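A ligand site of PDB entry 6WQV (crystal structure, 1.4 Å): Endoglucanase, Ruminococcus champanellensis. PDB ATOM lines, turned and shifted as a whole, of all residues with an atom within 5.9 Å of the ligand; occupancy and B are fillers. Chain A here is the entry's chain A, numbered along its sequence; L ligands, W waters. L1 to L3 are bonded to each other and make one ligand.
ND1 of His 241 lies within hydrogen-bond range of NE2 of Gln 164 (3.4 Å). The side-chain amide oxygen of Gln 288 is in hydrogen-bond range of the guanidinium group of Arg 75, 2.9 Å away. The side-chain amide oxygen (OD1) of Asn 323 lies within hydrogen-bond range of the backbone NH (N) of Phe 333 (3.0 Å). ND2 of Asn 323 is in hydrogen-bond range of O of Glu 331, 2.8 Å away. The side-chain amide nitrogen (ND2) of Asn 163 lies close to a ring nitrogen (NE2) of His 119, at 3.4 Å. NE2 of Gln 288 is in hydrogen-bond range of OH of Tyr 243. The backbone NH (N) of Asn 31 sits at hydrogen-bond distance from the side-chain carboxylate (OD2) of Asp 34. The side-chain amide oxygen of Asn 163 is in hydrogen-bond range of the guanidinium group of Arg 75, 2.9 Å away.
Residues that only touch the ligand: Gln 164, Trp 53, Tyr 243, Phe 333 and Leu 250. Hydrophobic or aromatic side chains that line the ligand: Trp 53, His 119, His 120, His 241, Tyr 243, Leu 250, Trp 321 and Phe 333.
The side-chain amide nitrogen (NE2) of Gln 288 lies within hydrogen-bond range of an oxygen (O1) of LIG L1. NE2 of His 119 sits at hydrogen-bond distance from O3 of LIG L1, 3.0 Å away. The indole nitrogen (NE1) of Trp 321 sits at hydrogen-bond distance from an oxygen (O1) of LG2 L2, at 3.1 Å. A ring nitrogen (ND1) of His 241 is in hydrogen-bond range of an oxygen (O1) of LIG L1 (2.9 Å). ND2 of Asn 163 lies within hydrogen-bond range of O2 of LIG L1. An oxygen (O3) of LIG L1 sits close to a ring nitrogen (NE2) of His 120, at 3.4 Å. O1 of LG2 L2 sits at hydrogen-bond distance from OE1 of Glu 331. The side-chain amide nitrogen (ND2) of Asn 31 sits at hydrogen-bond distance from an oxygen (O2) of LG2 L2 (2.9 Å). O1 of LG2 L2 sits at hydrogen-bond distance from ND2 of Asn 323, at 3.2 Å.
Water W8 lies within hydrogen-bond range of an oxygen (O2) of LG2 L2 and the backbone NH of Glu 331. Water W4 lies within hydrogen-bond range of the side-chain carboxylate of Asp 34 (2.7 Å), a ring nitrogen (NE2) of His 120 (2.8 Å), an oxygen (O3) of LIG L1 (2.9 Å) and the side-chain amide oxygen of Asn 31 (2.9 Å).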
ATOM      1  N   ASN A  31      17.103   7.188   0.603  1.00  0.00           N
ATOM      2  CA  ASN A  31      16.965   6.272   1.755  1.00  0.00           C
ATOM      3  C   ASN A  31      17.886   5.053   1.655  1.00  0.00           C
ATOM      4  O   ASN A  31      17.549   3.950   2.116  1.00  0.00           O
ATOM      5  CB  ASN A  31      15.507   5.841   1.962  1.00  0.00           C
ATOM      6  CG  ASN A  31      14.679   6.868   2.694  1.00  0.00           C
ATOM      7  OD1 ASN A  31      15.123   7.995   2.907  1.00  0.00           O
ATOM      8  ND2 ASN A  31      13.473   6.491   3.089  1.00  0.00           N
ATOM      9  N   ASP A  34      22.283   7.271   2.411  1.00  0.00           N
ATOM     10  CA  ASP A  34      21.904   8.329   3.347  1.00  0.00           C
ATOM     11  C   ASP A  34      21.251   7.802   4.620  1.00  0.00           C
ATOM     12  O   ASP A  34      21.057   8.578   5.561  1.00  0.00           O
ATOM     13  CB  ASP A  34      20.974   9.353   2.682  1.00  0.00           C
ATOM     14  CG  ASP A  34      19.847   8.716   1.834  1.00  0.00           C
ATOM     15  OD1 ASP A  34      20.122   7.789   1.043  1.00  0.00           O
ATOM     16  OD2 ASP A  34      18.686   9.181   1.963  1.00  0.00           O
ATOM     17  N   ALA A  52      19.154  -0.181   5.865  1.00  0.00           N
ATOM     18  CA  ALA A  52      18.489   0.121   7.126  1.00  0.00           C
ATOM     19  C   ALA A  52      17.099   0.704   6.944  1.00  0.00           C
ATOM     20  O   ALA A  52      16.268   0.586   7.851  1.00  0.00           O
ATOM     21  CB  ALA A  52      19.358   1.081   7.937  1.00  0.00           C
ATOM     22  N   TRP A  53      16.817   1.319   5.804  1.00  0.00           N
ATOM     23  CA  TRP A  53      15.574   2.067   5.598  1.00  0.00           C
ATOM     24  C   TRP A  53      14.787   1.537   4.396  1.00  0.00           C
ATOM     25  O   TRP A  53      14.306   2.313   3.560  1.00  0.00           O
ATOM     26  CB  TRP A  53      15.853   3.555   5.422  1.00  0.00           C
ATOM     27  CG  TRP A  53      16.242   4.326   6.661  1.00  0.00           C
ATOM     28  CD1 TRP A  53      16.331   3.866   7.939  1.00  0.00           C
ATOM     29  CD2 TRP A  53      16.606   5.714   6.697  1.00  0.00           C
ATOM     30  NE1 TRP A  53      16.723   4.885   8.773  1.00  0.00           N
ATOM     31  CE2 TRP A  53      16.891   6.028   8.044  1.00  0.00           C
ATOM     32  CE3 TRP A  53      16.715   6.716   5.730  1.00  0.00           C
ATOM     33  CZ2 TRP A  53      17.281   7.313   8.437  1.00  0.00           C
ATOM     34  CZ3 TRP A  53      17.102   7.986   6.130  1.00  0.00           C
ATOM     35  CH2 TRP A  53      17.383   8.273   7.470  1.00  0.00           C
ATOM     36  N   GLY A  54      14.663   0.233   4.276  1.00  0.00           N
ATOM     37  CA  GLY A  54      13.720  -0.345   3.329  1.00  0.00           C
ATOM     38  C   GLY A  54      14.203  -0.454   1.907  1.00  0.00           C
ATOM     39  O   GLY A  54      13.377  -0.665   1.005  1.00  0.00           O
ATOM     40  N   ARG A  75      21.613  11.560  -8.376  1.00  0.00           N
ATOM     41  CA  ARG A  75      22.132  12.108  -7.128  1.00  0.00           C
ATOM     42  C   ARG A  75      22.247  10.973  -6.130  1.00  0.00           C
ATOM     43  O   ARG A  75      21.282  10.211  -5.929  1.00  0.00           O
ATOM     44  CB  ARG A  75      21.214  13.206  -6.605  1.00  0.00           C
ATOM     45  CG  ARG A  75      21.677  13.831  -5.267  1.00  0.00           C
ATOM     46  CD  ARG A  75      21.012  15.168  -5.130  1.00  0.00           C
ATOM     47  NE  ARG A  75      21.240  15.967  -3.926  1.00  0.00           N
ATOM     48  CZ  ARG A  75      20.499  15.921  -2.828  1.00  0.00           C
ATOM     49  NH1 ARG A  75      19.505  15.045  -2.715  1.00  0.00           N
ATOM     50  NH2 ARG A  75      20.761  16.758  -1.842  1.00  0.00           N
ATOM     51  N   HIS A 119      24.915  14.129   3.614  1.00  0.00           N
ATOM     52  CA  HIS A 119      23.464  14.177   3.687  1.00  0.00           C
ATOM     53  C   HIS A 119      23.005  14.388   5.122  1.00  0.00           C
ATOM     54  O   HIS A 119      22.946  15.540   5.587  1.00  0.00           O
ATOM     55  CB  HIS A 119      22.838  12.971   2.963  1.00  0.00           C
ATOM     56  CG  HIS A 119      21.435  13.216   2.507  1.00  0.00           C
ATOM     57  ND1 HIS A 119      21.132  13.886   1.338  1.00  0.00           N
ATOM     58  CD2 HIS A 119      20.249  12.879   3.064  1.00  0.00           C
ATOM     59  CE1 HIS A 119      19.825  13.938   1.196  1.00  0.00           C
ATOM     60  NE2 HIS A 119      19.265  13.332   2.235  1.00  0.00           N
ATOM     61  N   HIS A 120      22.609  13.344   5.844  1.00  0.00           N
ATOM     62  CA  HIS A 120      22.041  13.521   7.189  1.00  0.00           C
ATOM     63  C   HIS A 120      23.158  13.636   8.233  1.00  0.00           C
ATOM     64  O   HIS A 120      23.390  12.744   9.051  1.00  0.00           O
ATOM     65  CB  HIS A 120      21.099  12.376   7.537  1.00  0.00           C
ATOM     66  CG  HIS A 120      19.863  12.314   6.701  1.00  0.00           C
ATOM     67  ND1 HIS A 120      19.082  13.418   6.435  1.00  0.00           N
ATOM     68  CD2 HIS A 120      19.245  11.263   6.096  1.00  0.00           C
ATOM     69  CE1 HIS A 120      18.038  13.057   5.703  1.00  0.00           C
ATOM     70  NE2 HIS A 120      18.117  11.750   5.480  1.00  0.00           N
ATOM     71  N   ASN A 163      23.556  19.106   2.549  1.00  0.00           N
ATOM     72  CA  ASN A 163      22.205  18.823   2.082  1.00  0.00           C
ATOM     73  C   ASN A 163      21.208  19.892   2.526  1.00  0.00           C
ATOM     74  O   ASN A 163      20.819  20.742   1.718  1.00  0.00           O
ATOM     75  CB  ASN A 163      21.767  17.438   2.559  1.00  0.00           C
ATOM     76  CG  ASN A 163      20.368  17.080   2.095  1.00  0.00           C
ATOM     77  OD1 ASN A 163      20.033  17.267   0.937  1.00  0.00           O
ATOM     78  ND2 ASN A 163      19.551  16.587   3.027  1.00  0.00           N
ATOM     79  N   GLN A 164      20.786  19.830   3.785  1.00  0.00           N
ATOM     80  CA  GLN A 164      19.777  20.754   4.329  1.00  0.00           C
ATOM     81  C   GLN A 164      20.240  21.289   5.677  1.00  0.00           C
ATOM     82  O   GLN A 164      19.602  21.044   6.708  1.00  0.00           O
ATOM     83  CB  GLN A 164      18.432  20.056   4.464  1.00  0.00           C
ATOM     84  CG  GLN A 164      17.715  19.852   3.173  1.00  0.00           C
ATOM     85  CD  GLN A 164      16.288  19.433   3.372  1.00  0.00           C
ATOM     86  OE1 GLN A 164      16.002  18.490   4.117  1.00  0.00           O
ATOM     87  NE2 GLN A 164      15.366  20.142   2.727  1.00  0.00           N
ATOM     88  N   TRP A 174      12.268  24.771   9.836  1.00  0.00           N
ATOM     89  CA  TRP A 174      11.900  24.676   8.427  1.00  0.00           C
ATOM     90  C   TRP A 174      11.298  25.972   7.908  1.00  0.00           C
ATOM     91  O   TRP A 174      10.530  25.958   6.939  1.00  0.00           O
ATOM     92  CB  TRP A 174      10.948  23.506   8.194  1.00  0.00           C
ATOM     93  CG  TRP A 174      11.491  22.180   8.603  1.00  0.00           C
ATOM     94  CD1 TRP A 174      11.168  21.467   9.710  1.00  0.00           C
ATOM     95  CD2 TRP A 174      12.458  21.390   7.895  1.00  0.00           C
ATOM     96  NE1 TRP A 174      11.865  20.289   9.753  1.00  0.00           N
ATOM     97  CE2 TRP A 174      12.673  20.223   8.639  1.00  0.00           C
ATOM     98  CE3 TRP A 174      13.180  21.570   6.705  1.00  0.00           C
ATOM     99  CZ2 TRP A 174      13.561  19.227   8.242  1.00  0.00           C
ATOM    100  CZ3 TRP A 174      14.063  20.583   6.300  1.00  0.00           C
ATOM    101  CH2 TRP A 174      14.244  19.422   7.077  1.00  0.00           C
ATOM    102  N   HIS A 241      15.692  22.389  -2.776  1.00  0.00           N
ATOM    103  CA  HIS A 241      14.681  21.332  -2.757  1.00  0.00           C
ATOM    104  C   HIS A 241      13.313  22.017  -2.761  1.00  0.00           C
ATOM    105  O   HIS A 241      13.092  22.987  -2.032  1.00  0.00           O
ATOM    106  CB  HIS A 241      14.815  20.448  -1.526  1.00  0.00           C
ATOM    107  CG  HIS A 241      16.173  19.840  -1.339  1.00  0.00           C
ATOM    108  ND1 HIS A 241      16.467  18.969  -0.310  1.00  0.00           N
ATOM    109  CD2 HIS A 241      17.317  19.990  -2.042  1.00  0.00           C
ATOM    110  CE1 HIS A 241      17.734  18.620  -0.381  1.00  0.00           C
ATOM    111  NE2 HIS A 241      18.285  19.220  -1.421  1.00  0.00           N
ATOM    112  N   TYR A 243       9.513  20.642  -2.796  1.00  0.00           N
ATOM    113  CA  TYR A 243       8.377  19.711  -2.788  1.00  0.00           C
ATOM    114  C   TYR A 243       7.109  20.560  -2.745  1.00  0.00           C
ATOM    115  O   TYR A 243       6.517  20.786  -1.686  1.00  0.00           O
ATOM    116  CB  TYR A 243       8.463  18.796  -1.575  1.00  0.00           C
ATOM    117  CG  TYR A 243       9.597  17.815  -1.588  1.00  0.00           C
ATOM    118  CD1 TYR A 243      10.872  18.173  -1.196  1.00  0.00           C
ATOM    119  CD2 TYR A 243       9.375  16.492  -1.938  1.00  0.00           C
ATOM    120  CE1 TYR A 243      11.909  17.253  -1.175  1.00  0.00           C
ATOM    121  CE2 TYR A 243      10.396  15.558  -1.910  1.00  0.00           C
ATOM    122  CZ  TYR A 243      11.667  15.944  -1.542  1.00  0.00           C
ATOM    123  OH  TYR A 243      12.674  15.014  -1.523  1.00  0.00           O
ATOM    124  N   LEU A 250       4.253  16.959  -0.065  1.00  0.00           N
ATOM    125  CA  LEU A 250       5.113  16.531   1.027  1.00  0.00           C
ATOM    126  C   LEU A 250       4.386  16.292   2.347  1.00  0.00           C
ATOM    127  O   LEU A 250       4.905  15.533   3.176  1.00  0.00           O
ATOM    128  CB  LEU A 250       6.235  17.549   1.255  1.00  0.00           C
ATOM    129  CG  LEU A 250       7.306  17.238   2.292  1.00  0.00           C
ATOM    130  CD1 LEU A 250       7.964  15.884   2.047  1.00  0.00           C
ATOM    131  CD2 LEU A 250       8.370  18.348   2.325  1.00  0.00           C
ATOM    132  N   GLN A 288      16.096  18.038  -5.251  1.00  0.00           N
ATOM    133  CA  GLN A 288      15.048  17.116  -4.841  1.00  0.00           C
ATOM    134  C   GLN A 288      13.685  17.743  -5.075  1.00  0.00           C
ATOM    135  O   GLN A 288      13.457  18.887  -4.674  1.00  0.00           O
ATOM    136  CB  GLN A 288      15.148  16.766  -3.351  1.00  0.00           C
ATOM    137  CG  GLN A 288      16.415  16.071  -2.918  1.00  0.00           C
ATOM    138  CD  GLN A 288      16.383  15.665  -1.441  1.00  0.00           C
ATOM    139  OE1 GLN A 288      17.421  15.513  -0.809  1.00  0.00           O
ATOM    140  NE2 GLN A 288      15.186  15.487  -0.898  1.00  0.00           N
ATOM    141  N   TRP A 321      13.083  12.652  -5.998  1.00  0.00           N
ATOM    142  CA  TRP A 321      13.491  11.962  -4.783  1.00  0.00           C
ATOM    143  C   TRP A 321      12.818  10.591  -4.734  1.00  0.00           C
ATOM    144  O   TRP A 321      11.603  10.512  -4.506  1.00  0.00           O
ATOM    145  CB  TRP A 321      13.121  12.779  -3.545  1.00  0.00           C
ATOM    146  CG  TRP A 321      13.432  12.090  -2.268  1.00  0.00           C
ATOM    147  CD1 TRP A 321      12.554  11.506  -1.408  1.00  0.00           C
ATOM    148  CD2 TRP A 321      14.732  11.897  -1.706  1.00  0.00           C
ATOM    149  NE1 TRP A 321      13.222  10.955  -0.346  1.00  0.00           N
ATOM    150  CE2 TRP A 321      14.572  11.192  -0.495  1.00  0.00           C
ATOM    151  CE3 TRP A 321      16.024  12.274  -2.101  1.00  0.00           C
ATOM    152  CZ2 TRP A 321      15.641  10.834   0.305  1.00  0.00           C
ATOM    153  CZ3 TRP A 321      17.087  11.924  -1.299  1.00  0.00           C
ATOM    154  CH2 TRP A 321      16.897  11.214  -0.109  1.00  0.00           C
ATOM    155  N   ASN A 323      12.651   7.176  -2.780  1.00  0.00           N
ATOM    156  CA  ASN A 323      13.006   6.426  -1.589  1.00  0.00           C
ATOM    157  C   ASN A 323      12.485   4.994  -1.606  1.00  0.00           C
ATOM    158  O   ASN A 323      12.477   4.338  -0.557  1.00  0.00           O
ATOM    159  CB  ASN A 323      12.550   7.145  -0.312  1.00  0.00           C
ATOM    160  CG  ASN A 323      11.053   7.208  -0.175  1.00  0.00           C
ATOM    161  OD1 ASN A 323      10.296   6.789  -1.053  1.00  0.00           O
ATOM    162  ND2 ASN A 323      10.597   7.731   0.964  1.00  0.00           N
ATOM    163  N   THR A 328       3.779   2.313   2.283  1.00  0.00           N
ATOM    164  CA  THR A 328       4.162   2.282   3.683  1.00  0.00           C
ATOM    165  C   THR A 328       3.383   3.331   4.472  1.00  0.00           C
ATOM    166  O   THR A 328       2.656   4.163   3.917  1.00  0.00           O
ATOM    167  CB  THR A 328       5.662   2.534   3.835  1.00  0.00           C
ATOM    168  OG1 THR A 328       5.927   3.936   3.660  1.00  0.00           O
ATOM    169  CG2 THR A 328       6.465   1.736   2.807  1.00  0.00           C
ATOM    170  N   GLY A 330       4.914   5.626   6.057  1.00  0.00           N
ATOM    171  CA  GLY A 330       5.775   6.784   5.999  1.00  0.00           C
ATOM    172  C   GLY A 330       5.600   7.562   4.712  1.00  0.00           C
ATOM    173  O   GLY A 330       4.516   7.596   4.114  1.00  0.00           O
ATOM    174  N   GLU A 331       6.683   8.211   4.279  1.00  0.00           N
ATOM    175  CA  GLU A 331       6.668   8.993   3.055  1.00  0.00           C
ATOM    176  C   GLU A 331       6.886   8.066   1.863  1.00  0.00           C
ATOM    177  O   GLU A 331       7.918   7.408   1.771  1.00  0.00           O
ATOM    178  CB  GLU A 331       7.768  10.051   3.097  1.00  0.00           C
ATOM    179  CG  GLU A 331       7.556  11.083   4.181  1.00  0.00           C
ATOM    180  CD  GLU A 331       8.655  12.125   4.291  1.00  0.00           C
ATOM    181  OE1 GLU A 331       9.609  12.136   3.472  1.00  0.00           O
ATOM    182  OE2 GLU A 331       8.557  12.962   5.216  1.00  0.00           O
ATOM    183  N   PHE A 333       7.640   8.028  -1.658  1.00  0.00           N
ATOM    184  CA  PHE A 333       8.172   8.718  -2.821  1.00  0.00           C
ATOM    185  C   PHE A 333       8.728   7.769  -3.875  1.00  0.00           C
ATOM    186  O   PHE A 333       9.415   8.202  -4.800  1.00  0.00           O
ATOM    187  CB  PHE A 333       9.243   9.729  -2.400  1.00  0.00           C
ATOM    188  CG  PHE A 333       8.698  10.991  -1.776  1.00  0.00           C
ATOM    189  CD1 PHE A 333       7.992  11.912  -2.537  1.00  0.00           C
ATOM    190  CD2 PHE A 333       8.951  11.285  -0.445  1.00  0.00           C
ATOM    191  CE1 PHE A 333       7.518  13.085  -1.965  1.00  0.00           C
ATOM    192  CE2 PHE A 333       8.471  12.466   0.129  1.00  0.00           C
ATOM    193  CZ  PHE A 333       7.752  13.354  -0.639  1.00  0.00           C
HETATM  194  C1  LIG L   1      14.724  16.467   2.227  1.00  0.00           C
HETATM  195  C2  LIG L   1      15.746  15.385   2.508  1.00  0.00           C
HETATM  196  C3  LIG L   1      15.413  13.975   2.230  1.00  0.00           C
HETATM  197  C4  LIG L   1      14.026  13.657   2.720  1.00  0.00           C
HETATM  198  C5  LIG L   1      13.080  14.553   1.954  1.00  0.00           C
HETATM  199  C6  LIG L   1      11.602  14.225   2.143  1.00  0.00           C
HETATM  200  O1  LIG L   1      14.759  17.057   0.999  1.00  0.00           O
HETATM  201  O2  LIG L   1      16.983  15.797   1.845  1.00  0.00           O
HETATM  202  O3  LIG L   1      16.404  13.148   2.951  1.00  0.00           O
HETATM  203  O4  LIG L   1      13.756  12.268   2.498  1.00  0.00           O
HETATM  204  O5  LIG L   1      13.290  15.960   2.395  1.00  0.00           O
HETATM  205  O6  LIG L   1      11.213  14.407   3.439  1.00  0.00           O
HETATM  206  C1  LG2 L   2      12.540  10.385   3.239  1.00  0.00           C
HETATM  207  C2  LG2 L   2      11.976   9.711   4.447  1.00  0.00           C
HETATM  208  C3  LG2 L   2      12.986   9.592   5.559  1.00  0.00           C
HETATM  209  C4  LG2 L   2      13.591  10.933   5.904  1.00  0.00           C
HETATM  210  C5  LG2 L   2      14.718  10.904   6.893  1.00  0.00           C
HETATM  211  C6  LG2 L   2      13.138  11.735   3.585  1.00  0.00           C
HETATM  212  O1  LG2 L   2      11.519  10.548   2.229  1.00  0.00           O
HETATM  213  O2  LG2 L   2      11.500   8.372   4.062  1.00  0.00           O
HETATM  214  O3  LG2 L   2      12.327   9.119   6.794  1.00  0.00           O
HETATM  215  O4  LG2 L   2      14.145  11.555   4.673  1.00  0.00           O
HETATM  216  O5  LG2 L   2      15.051  12.238   7.277  1.00  0.00           O
HETATM  217  C1  LG3 L   3      12.582   7.913   8.812  1.00  0.00           C
HETATM  218  C2  LG3 L   3      13.041   6.640   9.429  1.00  0.00           C
HETATM  219  C3  LG3 L   3      12.550   5.427   8.673  1.00  0.00           C
HETATM  220  C4  LG3 L   3      12.928   5.535   7.188  1.00  0.00           C
HETATM  221  C5  LG3 L   3      12.349   4.368   6.392  1.00  0.00           C
HETATM  222  C6  LG3 L   3      12.930   8.006   7.345  1.00  0.00           C
HETATM  223  O1  LG3 L   3      13.172   9.044   9.467  1.00  0.00           O
HETATM  224  O2  LG3 L   3      12.546   6.588  10.793  1.00  0.00           O
HETATM  225  O3  LG3 L   3      13.150   4.250   9.220  1.00  0.00           O
HETATM  226  O4  LG3 L   3      12.409   6.778   6.616  1.00  0.00           O
HETATM  227  O5  LG3 L   3      10.959   4.522   6.314  1.00  0.00           O
HETATM  228  O   HOH W   1      10.400   3.654   3.975  1.00  0.00           O
HETATM  229  O   HOH W   2      16.730  12.426   9.303  1.00  0.00           O
HETATM  230  O   HOH W   3      15.013  14.927   6.375  1.00  0.00           O
HETATM  231  O   HOH W   4      16.780  10.337   3.444  1.00  0.00           O
HETATM  232  O   HOH W   5      12.288   0.955   6.939  1.00  0.00           O
HETATM  233  O   HOH W   6      12.169  15.785   5.610  1.00  0.00           O
HETATM  234  O   HOH W   7       9.057   9.929   7.701  1.00  0.00           O
HETATM  235  O   HOH W   8       9.255   7.889   5.683  1.00  0.00           O
HETATM  236  O   HOH W   9      15.415   9.387  10.934  1.00  0.00           O
